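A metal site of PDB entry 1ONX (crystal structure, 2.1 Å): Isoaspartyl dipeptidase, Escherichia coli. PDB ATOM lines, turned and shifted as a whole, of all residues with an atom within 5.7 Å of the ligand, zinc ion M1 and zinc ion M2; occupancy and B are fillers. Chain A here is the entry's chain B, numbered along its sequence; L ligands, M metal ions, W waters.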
ATOM      1  N   HIS A  68     -33.637  17.792  24.873  1.00  0.00           N
ATOM      2  CA  HIS A  68     -32.710  18.922  24.906  1.00  0.00           C
ATOM      3  C   HIS A  68     -33.246  20.087  24.105  1.00  0.00           C
ATOM      4  O   HIS A  68     -32.858  20.278  22.975  1.00  0.00           O
ATOM      5  CB  HIS A  68     -31.332  18.533  24.368  1.00  0.00           C
ATOM      6  CG  HIS A  68     -30.234  19.413  24.861  1.00  0.00           C
ATOM      7  ND1 HIS A  68     -29.288  18.943  25.750  1.00  0.00           N
ATOM      8  CD2 HIS A  68     -29.917  20.691  24.567  1.00  0.00           C
ATOM      9  CE1 HIS A  68     -28.443  19.927  26.011  1.00  0.00           C
ATOM     10  NE2 HIS A  68     -28.814  20.996  25.334  1.00  0.00           N
ATOM     11  N   HIS A  70     -34.146  24.374  23.998  1.00  0.00           N
ATOM     12  CA  HIS A  70     -34.157  25.681  24.593  1.00  0.00           C
ATOM     13  C   HIS A  70     -35.523  26.310  24.404  1.00  0.00           C
ATOM     14  O   HIS A  70     -35.759  27.194  23.563  1.00  0.00           O
ATOM     15  CB  HIS A  70     -33.032  26.535  23.992  1.00  0.00           C
ATOM     16  CG  HIS A  70     -31.752  25.880  24.380  1.00  0.00           C
ATOM     17  ND1 HIS A  70     -31.003  26.343  25.454  1.00  0.00           N
ATOM     18  CD2 HIS A  70     -31.147  24.836  23.844  1.00  0.00           C
ATOM     19  CE1 HIS A  70     -29.926  25.590  25.522  1.00  0.00           C
ATOM     20  NE2 HIS A  70     -29.991  24.702  24.558  1.00  0.00           N
ATOM     21  N   GLY A  73     -35.867  30.090  24.375  1.00  0.00           N
ATOM     22  CA  GLY A  73     -34.868  30.729  23.549  1.00  0.00           C
ATOM     23  C   GLY A  73     -33.512  30.587  24.252  1.00  0.00           C
ATOM     24  O   GLY A  73     -33.432  30.140  25.407  1.00  0.00           O
ATOM     25  N   GLY A  74     -32.419  30.898  23.587  1.00  0.00           N
ATOM     26  CA  GLY A  74     -31.119  30.763  24.210  1.00  0.00           C
ATOM     27  C   GLY A  74     -30.168  31.749  23.586  1.00  0.00           C
ATOM     28  O   GLY A  74     -30.558  32.894  23.395  1.00  0.00           O
ATOM     29  N   GLY A  75     -28.948  31.271  23.311  1.00  0.00           N
ATOM     30  CA  GLY A  75     -27.917  32.082  22.682  1.00  0.00           C
ATOM     31  C   GLY A  75     -27.449  33.215  23.588  1.00  0.00           C
ATOM     32  O   GLY A  75     -27.515  33.111  24.833  1.00  0.00           O
ATOM     33  N   GLU A  77     -24.308  34.401  23.169  1.00  0.00           N
ATOM     34  CA  GLU A  77     -22.823  34.346  23.208  1.00  0.00           C
ATOM     35  C   GLU A  77     -22.082  35.495  22.534  1.00  0.00           C
ATOM     36  O   GLU A  77     -20.949  35.850  22.872  1.00  0.00           O
ATOM     37  CB  GLU A  77     -22.257  33.007  22.726  1.00  0.00           C
ATOM     38  CG  GLU A  77     -22.600  31.851  23.684  1.00  0.00           C
ATOM     39  CD  GLU A  77     -23.792  31.057  23.272  1.00  0.00           C
ATOM     40  OE1 GLU A  77     -24.638  31.450  22.499  1.00  0.00           O
ATOM     41  OE2 GLU A  77     -23.801  29.913  23.875  1.00  0.00           O
ATOM     42  N   THR A  84     -31.760  33.862  21.130  1.00  0.00           N
ATOM     43  CA  THR A  84     -32.731  33.205  20.248  1.00  0.00           C
ATOM     44  C   THR A  84     -34.155  33.303  20.795  1.00  0.00           C
ATOM     45  O   THR A  84     -34.402  33.413  21.992  1.00  0.00           O
ATOM     46  CB  THR A  84     -32.306  31.771  19.914  1.00  0.00           C
ATOM     47  OG1 THR A  84     -32.193  31.053  21.123  1.00  0.00           O
ATOM     48  CG2 THR A  84     -30.879  31.723  19.324  1.00  0.00           C
ATOM     49  N   LEU A 103     -34.482  23.256  28.946  1.00  0.00           N
ATOM     50  CA  LEU A 103     -33.351  23.654  29.735  1.00  0.00           C
ATOM     51  C   LEU A 103     -32.806  25.015  29.310  1.00  0.00           C
ATOM     52  O   LEU A 103     -33.236  25.617  28.341  1.00  0.00           O
ATOM     53  CB  LEU A 103     -32.245  22.580  29.699  1.00  0.00           C
ATOM     54  CG  LEU A 103     -32.048  22.088  28.283  1.00  0.00           C
ATOM     55  CD1 LEU A 103     -31.439  23.159  27.399  1.00  0.00           C
ATOM     56  CD2 LEU A 103     -31.211  20.807  28.300  1.00  0.00           C
ATOM     57  N   LEU A 104     -31.844  25.494  30.105  1.00  0.00           N
ATOM     58  CA  LEU A 104     -31.164  26.739  29.849  1.00  0.00           C
ATOM     59  C   LEU A 104     -29.766  26.416  29.386  1.00  0.00           C
ATOM     60  O   LEU A 104     -29.346  25.273  29.488  1.00  0.00           O
ATOM     61  CB  LEU A 104     -31.132  27.714  31.064  1.00  0.00           C
ATOM     62  CG  LEU A 104     -32.538  28.149  31.505  1.00  0.00           C
ATOM     63  CD1 LEU A 104     -32.401  29.229  32.552  1.00  0.00           C
ATOM     64  CD2 LEU A 104     -33.367  28.664  30.332  1.00  0.00           C
ATOM     65  N   GLY A 105     -29.052  27.411  28.878  1.00  0.00           N
ATOM     66  CA  GLY A 105     -27.706  27.227  28.392  1.00  0.00           C
ATOM     67  C   GLY A 105     -26.673  28.165  29.008  1.00  0.00           C
ATOM     68  O   GLY A 105     -26.448  28.228  30.202  1.00  0.00           O
ATOM     69  N   THR A 106     -25.964  28.837  28.128  1.00  0.00           N
ATOM     70  CA  THR A 106     -24.886  29.697  28.555  1.00  0.00           C
ATOM     71  C   THR A 106     -25.335  30.864  29.405  1.00  0.00           C
ATOM     72  O   THR A 106     -24.739  31.189  30.420  1.00  0.00           O
ATOM     73  CB  THR A 106     -24.149  30.201  27.301  1.00  0.00           C
ATOM     74  OG1 THR A 106     -23.827  29.061  26.536  1.00  0.00           O
ATOM     75  CG2 THR A 106     -22.865  30.943  27.681  1.00  0.00           C
ATOM     76  N   ASP A 107     -26.374  31.531  28.951  1.00  0.00           N
ATOM     77  CA  ASP A 107     -26.905  32.669  29.629  1.00  0.00           C
ATOM     78  C   ASP A 107     -27.985  32.317  30.660  1.00  0.00           C
ATOM     79  O   ASP A 107     -29.031  31.742  30.377  1.00  0.00           O
ATOM     80  CB  ASP A 107     -27.524  33.626  28.553  1.00  0.00           C
ATOM     81  CG  ASP A 107     -28.180  34.865  29.145  1.00  0.00           C
ATOM     82  OD1 ASP A 107     -28.235  35.066  30.347  1.00  0.00           O
ATOM     83  OD2 ASP A 107     -28.720  35.670  28.235  1.00  0.00           O
ATOM     84  N   TYR A 137     -25.674  26.445  32.525  1.00  0.00           N
ATOM     85  CA  TYR A 137     -24.233  26.188  32.468  1.00  0.00           C
ATOM     86  C   TYR A 137     -23.582  26.398  33.840  1.00  0.00           C
ATOM     87  O   TYR A 137     -22.813  25.564  34.323  1.00  0.00           O
ATOM     88  CB  TYR A 137     -23.531  27.164  31.531  1.00  0.00           C
ATOM     89  CG  TYR A 137     -23.456  26.691  30.091  1.00  0.00           C
ATOM     90  CD1 TYR A 137     -24.464  25.898  29.529  1.00  0.00           C
ATOM     91  CD2 TYR A 137     -22.341  27.019  29.313  1.00  0.00           C
ATOM     92  CE1 TYR A 137     -24.405  25.482  28.198  1.00  0.00           C
ATOM     93  CE2 TYR A 137     -22.273  26.618  27.971  1.00  0.00           C
ATOM     94  CZ  TYR A 137     -23.307  25.852  27.425  1.00  0.00           C
ATOM     95  OH  TYR A 137     -23.203  25.484  26.124  1.00  0.00           O
ATOM     96  N   KCX A 162     -29.132  20.747  35.104  1.00  0.00           N
ATOM     97  CA  KCX A 162     -28.228  20.874  33.987  1.00  0.00           C
ATOM     98  CB  KCX A 162     -28.956  21.729  32.961  1.00  0.00           C
ATOM     99  CG  KCX A 162     -28.039  22.395  31.944  1.00  0.00           C
ATOM    100  CD  KCX A 162     -27.769  21.495  30.751  1.00  0.00           C
ATOM    101  CE  KCX A 162     -26.801  22.068  29.763  1.00  0.00           C
ATOM    102  NZ  KCX A 162     -27.498  22.923  28.803  1.00  0.00           N
ATOM    103  C   KCX A 162     -26.980  21.600  34.429  1.00  0.00           C
ATOM    104  O   KCX A 162     -27.064  22.438  35.325  1.00  0.00           O
ATOM    105  CX  KCX A 162     -26.921  22.751  27.458  1.00  0.00           C
ATOM    106  OQ1 KCX A 162     -27.411  23.628  26.615  1.00  0.00           O
ATOM    107  OQ2 KCX A 162     -26.080  21.902  27.176  1.00  0.00           O
ATOM    108  N   ARG A 169     -16.898  28.075  28.293  1.00  0.00           N
ATOM    109  CA  ARG A 169     -18.003  28.918  28.782  1.00  0.00           C
ATOM    110  C   ARG A 169     -18.541  28.402  30.135  1.00  0.00           C
ATOM    111  O   ARG A 169     -19.600  28.791  30.640  1.00  0.00           O
ATOM    112  CB  ARG A 169     -19.138  28.856  27.804  1.00  0.00           C
ATOM    113  CG  ARG A 169     -18.798  29.515  26.461  1.00  0.00           C
ATOM    114  CD  ARG A 169     -19.850  29.082  25.437  1.00  0.00           C
ATOM    115  NE  ARG A 169     -19.769  27.636  25.273  1.00  0.00           N
ATOM    116  CZ  ARG A 169     -20.445  26.931  24.365  1.00  0.00           C
ATOM    117  NH1 ARG A 169     -21.313  27.498  23.529  1.00  0.00           N
ATOM    118  NH2 ARG A 169     -20.285  25.606  24.329  1.00  0.00           N
ATOM    119  N   HIS A 201     -23.516  19.357  29.813  1.00  0.00           N
ATOM    120  CA  HIS A 201     -23.256  19.922  28.500  1.00  0.00           C
ATOM    121  C   HIS A 201     -21.760  19.773  28.374  1.00  0.00           C
ATOM    122  O   HIS A 201     -21.031  20.280  29.240  1.00  0.00           O
ATOM    123  CB  HIS A 201     -23.512  21.461  28.465  1.00  0.00           C
ATOM    124  CG  HIS A 201     -22.575  22.193  27.521  1.00  0.00           C
ATOM    125  ND1 HIS A 201     -22.974  22.457  26.212  1.00  0.00           N
ATOM    126  CD2 HIS A 201     -21.257  22.634  27.655  1.00  0.00           C
ATOM    127  CE1 HIS A 201     -21.947  23.046  25.593  1.00  0.00           C
ATOM    128  NE2 HIS A 201     -20.889  23.175  26.423  1.00  0.00           N
ATOM    129  N   MET A 202     -21.298  19.119  27.312  1.00  0.00           N
ATOM    130  CA  MET A 202     -19.867  18.974  27.173  1.00  0.00           C
ATOM    131  C   MET A 202     -19.347  19.921  26.131  1.00  0.00           C
ATOM    132  O   MET A 202     -19.956  20.118  25.069  1.00  0.00           O
ATOM    133  CB  MET A 202     -19.511  17.570  26.686  1.00  0.00           C
ATOM    134  CG  MET A 202     -20.197  16.532  27.529  1.00  0.00           C
ATOM    135  SD  MET A 202     -19.372  16.414  29.113  1.00  0.00           S
ATOM    136  CE  MET A 202     -17.631  16.598  28.662  1.00  0.00           C
ATOM    137  N   THR A 229     -23.985  15.077  27.263  1.00  0.00           N
ATOM    138  CA  THR A 229     -24.626  15.373  25.981  1.00  0.00           C
ATOM    139  C   THR A 229     -23.671  16.000  24.981  1.00  0.00           C
ATOM    140  O   THR A 229     -22.608  16.469  25.400  1.00  0.00           O
ATOM    141  CB  THR A 229     -25.933  16.172  26.190  1.00  0.00           C
ATOM    142  OG1 THR A 229     -26.517  16.260  24.914  1.00  0.00           O
ATOM    143  CG2 THR A 229     -25.707  17.584  26.772  1.00  0.00           C
ATOM    144  N   HIS A 230     -24.061  16.051  23.707  1.00  0.00           N
ATOM    145  CA  HIS A 230     -23.196  16.600  22.652  1.00  0.00           C
ATOM    146  C   HIS A 230     -21.976  15.729  22.480  1.00  0.00           C
ATOM    147  O   HIS A 230     -20.914  16.244  22.119  1.00  0.00           O
ATOM    148  CB  HIS A 230     -22.599  17.974  23.019  1.00  0.00           C
ATOM    149  CG  HIS A 230     -23.589  18.995  23.453  1.00  0.00           C
ATOM    150  ND1 HIS A 230     -24.848  19.120  22.870  1.00  0.00           N
ATOM    151  CD2 HIS A 230     -23.465  19.962  24.404  1.00  0.00           C
ATOM    152  CE1 HIS A 230     -25.467  20.105  23.483  1.00  0.00           C
ATOM    153  NE2 HIS A 230     -24.645  20.634  24.385  1.00  0.00           N
ATOM    154  N   ARG A 233     -19.441  15.980  19.452  1.00  0.00           N
ATOM    155  CA  ARG A 233     -18.779  17.231  19.109  1.00  0.00           C
ATOM    156  C   ARG A 233     -17.295  17.083  18.738  1.00  0.00           C
ATOM    157  O   ARG A 233     -16.707  17.880  18.011  1.00  0.00           O
ATOM    158  CB  ARG A 233     -19.034  18.326  20.164  1.00  0.00           C
ATOM    159  CG  ARG A 233     -18.554  17.927  21.547  1.00  0.00           C
ATOM    160  CD  ARG A 233     -18.572  19.102  22.515  1.00  0.00           C
ATOM    161  NE  ARG A 233     -18.455  20.355  21.790  1.00  0.00           N
ATOM    162  CZ  ARG A 233     -19.270  21.398  21.881  1.00  0.00           C
ATOM    163  NH1 ARG A 233     -20.294  21.467  22.743  1.00  0.00           N
ATOM    164  NH2 ARG A 233     -19.022  22.466  21.125  1.00  0.00           N
ATOM    165  N   ASP A 285     -31.286  19.927  20.643  1.00  0.00           N
ATOM    166  CA  ASP A 285     -30.624  21.154  21.110  1.00  0.00           C
ATOM    167  C   ASP A 285     -31.326  22.315  20.390  1.00  0.00           C
ATOM    168  O   ASP A 285     -30.751  23.384  20.220  1.00  0.00           O
ATOM    169  CB  ASP A 285     -29.100  21.231  20.804  1.00  0.00           C
ATOM    170  CG  ASP A 285     -28.354  22.214  21.682  1.00  0.00           C
ATOM    171  OD1 ASP A 285     -28.905  22.846  22.574  1.00  0.00           O
ATOM    172  OD2 ASP A 285     -27.068  22.300  21.433  1.00  0.00           O
ATOM    173  N   ASN A 287     -33.406  25.399  19.077  1.00  0.00           N
ATOM    174  CA  ASN A 287     -33.491  26.794  19.478  1.00  0.00           C
ATOM    175  C   ASN A 287     -32.315  27.370  20.191  1.00  0.00           C
ATOM    176  O   ASN A 287     -32.397  28.473  20.646  1.00  0.00           O
ATOM    177  CB  ASN A 287     -34.797  27.184  20.178  1.00  0.00           C
ATOM    178  CG  ASN A 287     -35.785  27.712  19.159  1.00  0.00           C
ATOM    179  OD1 ASN A 287     -35.821  27.269  17.998  1.00  0.00           O
ATOM    180  ND2 ASN A 287     -36.586  28.685  19.614  1.00  0.00           N
ATOM    181  N   GLY A 288     -31.238  26.605  20.300  1.00  0.00           N
ATOM    182  CA  GLY A 288     -30.046  27.077  20.898  1.00  0.00           C
ATOM    183  C   GLY A 288     -29.200  27.658  19.772  1.00  0.00           C
ATOM    184  O   GLY A 288     -29.524  27.535  18.582  1.00  0.00           O
ATOM    185  N   SER A 289     -28.109  28.297  20.127  1.00  0.00           N
ATOM    186  CA  SER A 289     -27.308  28.816  19.070  1.00  0.00           C
ATOM    187  C   SER A 289     -26.227  27.814  18.723  1.00  0.00           C
ATOM    188  O   SER A 289     -25.891  26.959  19.559  1.00  0.00           O
ATOM    189  CB  SER A 289     -26.679  30.136  19.427  1.00  0.00           C
ATOM    190  OG  SER A 289     -25.865  29.958  20.560  1.00  0.00           O
ATOM    191  N   GLN A 290     -25.765  27.948  17.500  1.00  0.00           N
ATOM    192  CA  GLN A 290     -24.654  27.197  16.952  1.00  0.00           C
ATOM    193  C   GLN A 290     -23.494  28.177  16.837  1.00  0.00           C
ATOM    194  O   GLN A 290     -23.273  28.859  15.815  1.00  0.00           O
ATOM    195  CB  GLN A 290     -25.020  26.442  15.639  1.00  0.00           C
ATOM    196  CG  GLN A 290     -25.993  25.247  15.728  1.00  0.00           C
ATOM    197  CD  GLN A 290     -26.944  25.069  14.510  1.00  0.00           C
ATOM    198  OE1 GLN A 290     -27.863  24.227  14.526  1.00  0.00           O
ATOM    199  NE2 GLN A 290     -26.692  25.810  13.425  1.00  0.00           N
ATOM    200  N   PRO A 291     -22.828  28.343  18.001  1.00  0.00           N
ATOM    201  CA  PRO A 291     -21.673  29.226  18.115  1.00  0.00           C
ATOM    202  C   PRO A 291     -20.435  28.470  17.713  1.00  0.00           C
ATOM    203  O   PRO A 291     -20.272  27.298  18.016  1.00  0.00           O
ATOM    204  CB  PRO A 291     -21.559  29.626  19.597  1.00  0.00           C
ATOM    205  CG  PRO A 291     -22.539  28.742  20.343  1.00  0.00           C
ATOM    206  CD  PRO A 291     -23.252  27.878  19.333  1.00  0.00           C
HETATM  207  N1  LIG L   1     -25.518  27.641  22.639  1.00  0.00           N
HETATM  208  C1  LIG L   1     -26.481  27.148  23.453  1.00  0.00           C
HETATM  209  C2  LIG L   1     -27.369  28.200  24.082  1.00  0.00           C
HETATM  210  O1  LIG L   1     -27.120  28.577  25.258  1.00  0.00           O
HETATM  211  C3  LIG L   1     -25.887  26.436  24.682  1.00  0.00           C
HETATM  212  C4  LIG L   1     -25.622  25.025  24.320  1.00  0.00           C
HETATM  213  O2  LIG L   1     -24.977  24.291  25.014  1.00  0.00           O
HETATM  214  O3  LIG L   1     -26.150  24.680  23.179  1.00  0.00           O
HETATM  215  O4  LIG L   1     -28.328  28.676  23.425  1.00  0.00           O
HETATM  216 ZN    ZN M   1     -24.754  22.407  25.525  1.00  0.00          ZN
HETATM  217 ZN    ZN M   2     -28.232  23.256  24.605  1.00  0.00          ZN
HETATM  218  O   HOH W   1     -27.896  30.942  26.579  1.00  0.00           O
HETATM  219  O   HOH W   2     -22.840  24.611  22.204  1.00  0.00           O
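An oxygen (O3) of the ligand lies close to the side-chain carboxylate (OD2) of Asp 285 (3.1 Å). An oxygen (O2) of the ligand lies close to the side-chain hydroxyl (OH) of Tyr 137, 2.4 Å away. N of Gly 75 sits at hydrogen-bond distance from O4 of the ligand, at 2.7 Å. N1 of the ligand is in salt-bridge range of OE2 of Glu 77. N of Thr 106 lies within hydrogen-bond range of O1 of the ligand, at 3.1 Å. The backbone NH of Ser 289 sits at hydrogen-bond distance from an oxygen (O4) of the ligand, 3.3 Å away. O of Ser 289 sits at hydrogen-bond distance from N1 of the ligand (3.2 Å). OG of Ser 289 lies within hydrogen-bond range of N1 of the ligand, 3.1 Å away.
Zinc ion M1 is bound by ND1 of His 201 (1.9 Å), O2 of the ligand (2.0 Å), NE2 of His 230 (2.1 Å) and OQ2 of KCX 162 (2.2 Å). Zinc ion M1 has four donor atoms within binding distance.
The side-chain hydroxyl of Tyr 137 sits close to a ring nitrogen (NE2) of His 201, 3.3 Å away. A ring nitrogen (NE2) of His 201 is in hydrogen-bond range of the guanidinium group (NH2) of Arg 169 (3.3 Å). NZ of KCX 162 sits at hydrogen-bond distance from the backbone carbonyl oxygen (O) of Leu 104, 3.1 Å away. The backbone NH (N) of Tyr 137 sits at hydrogen-bond distance from the backbone carbonyl oxygen (O) of Gly 105 (3.0 Å). OH of Tyr 137 is in hydrogen-bond range of NH2 of Arg 169 (3.4 Å). The side-chain carboxylate (OE2) of Glu 77 lies within hydrogen-bond range of the side-chain hydroxyl (OG1) of Thr 106, at 2.8 Å. OE1 of Glu 77 sits at hydrogen-bond distance from OG of Ser 289, 2.7 Å away. The guanidinium group (NH1) of Arg 169 is in salt-bridge range of the side-chain carboxylate (OE2) of Glu 77.
Zinc ion M2 is bound by OD1 of Asp 285, OQ1 of KCX 162, NE2 of His 70 and NE2 of His 68. Zinc ion M2 has four donor atoms within binding distance.
The nearest printed residue that does not touch zinc ion M2 is Leu 103 (4.3 Å).
OH of Tyr 137 touches zinc ion M1 (3.5 Å). Four residues have an atom within 4 Å of zinc ion M1: Tyr 137, KCX 162, His 201 and His 230. The nearest printed residue that does not touch zinc ion M1 is His 68 (4.3 Å).
Gly 74 touches the ligand. CA of Gly 105 touches O1 of the ligand, 3.5 Å away. Gly 288 touches the ligand (CA to O4, 3.4 Å). CG of Pro 291 touches N1 of the ligand (3.9 Å). Hydrophobic or aromatic side chains that line the ligand: His 70, Tyr 137, His 201 and Pro 291. Of the 26 residues printed, 14 come within 4 Å of the ligand.
Water W1 lies within hydrogen-bond range of O of Gly 75 (2.8 Å), O1 of the ligand (2.8 Å), N of Asp 107 (2.9 Å) and N of Thr 106 (3.3 Å). Water W2 bridges an oxygen (O3) of the ligand (3.5 Å) and the guanidinium group of Arg 169 (3.5 Å).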
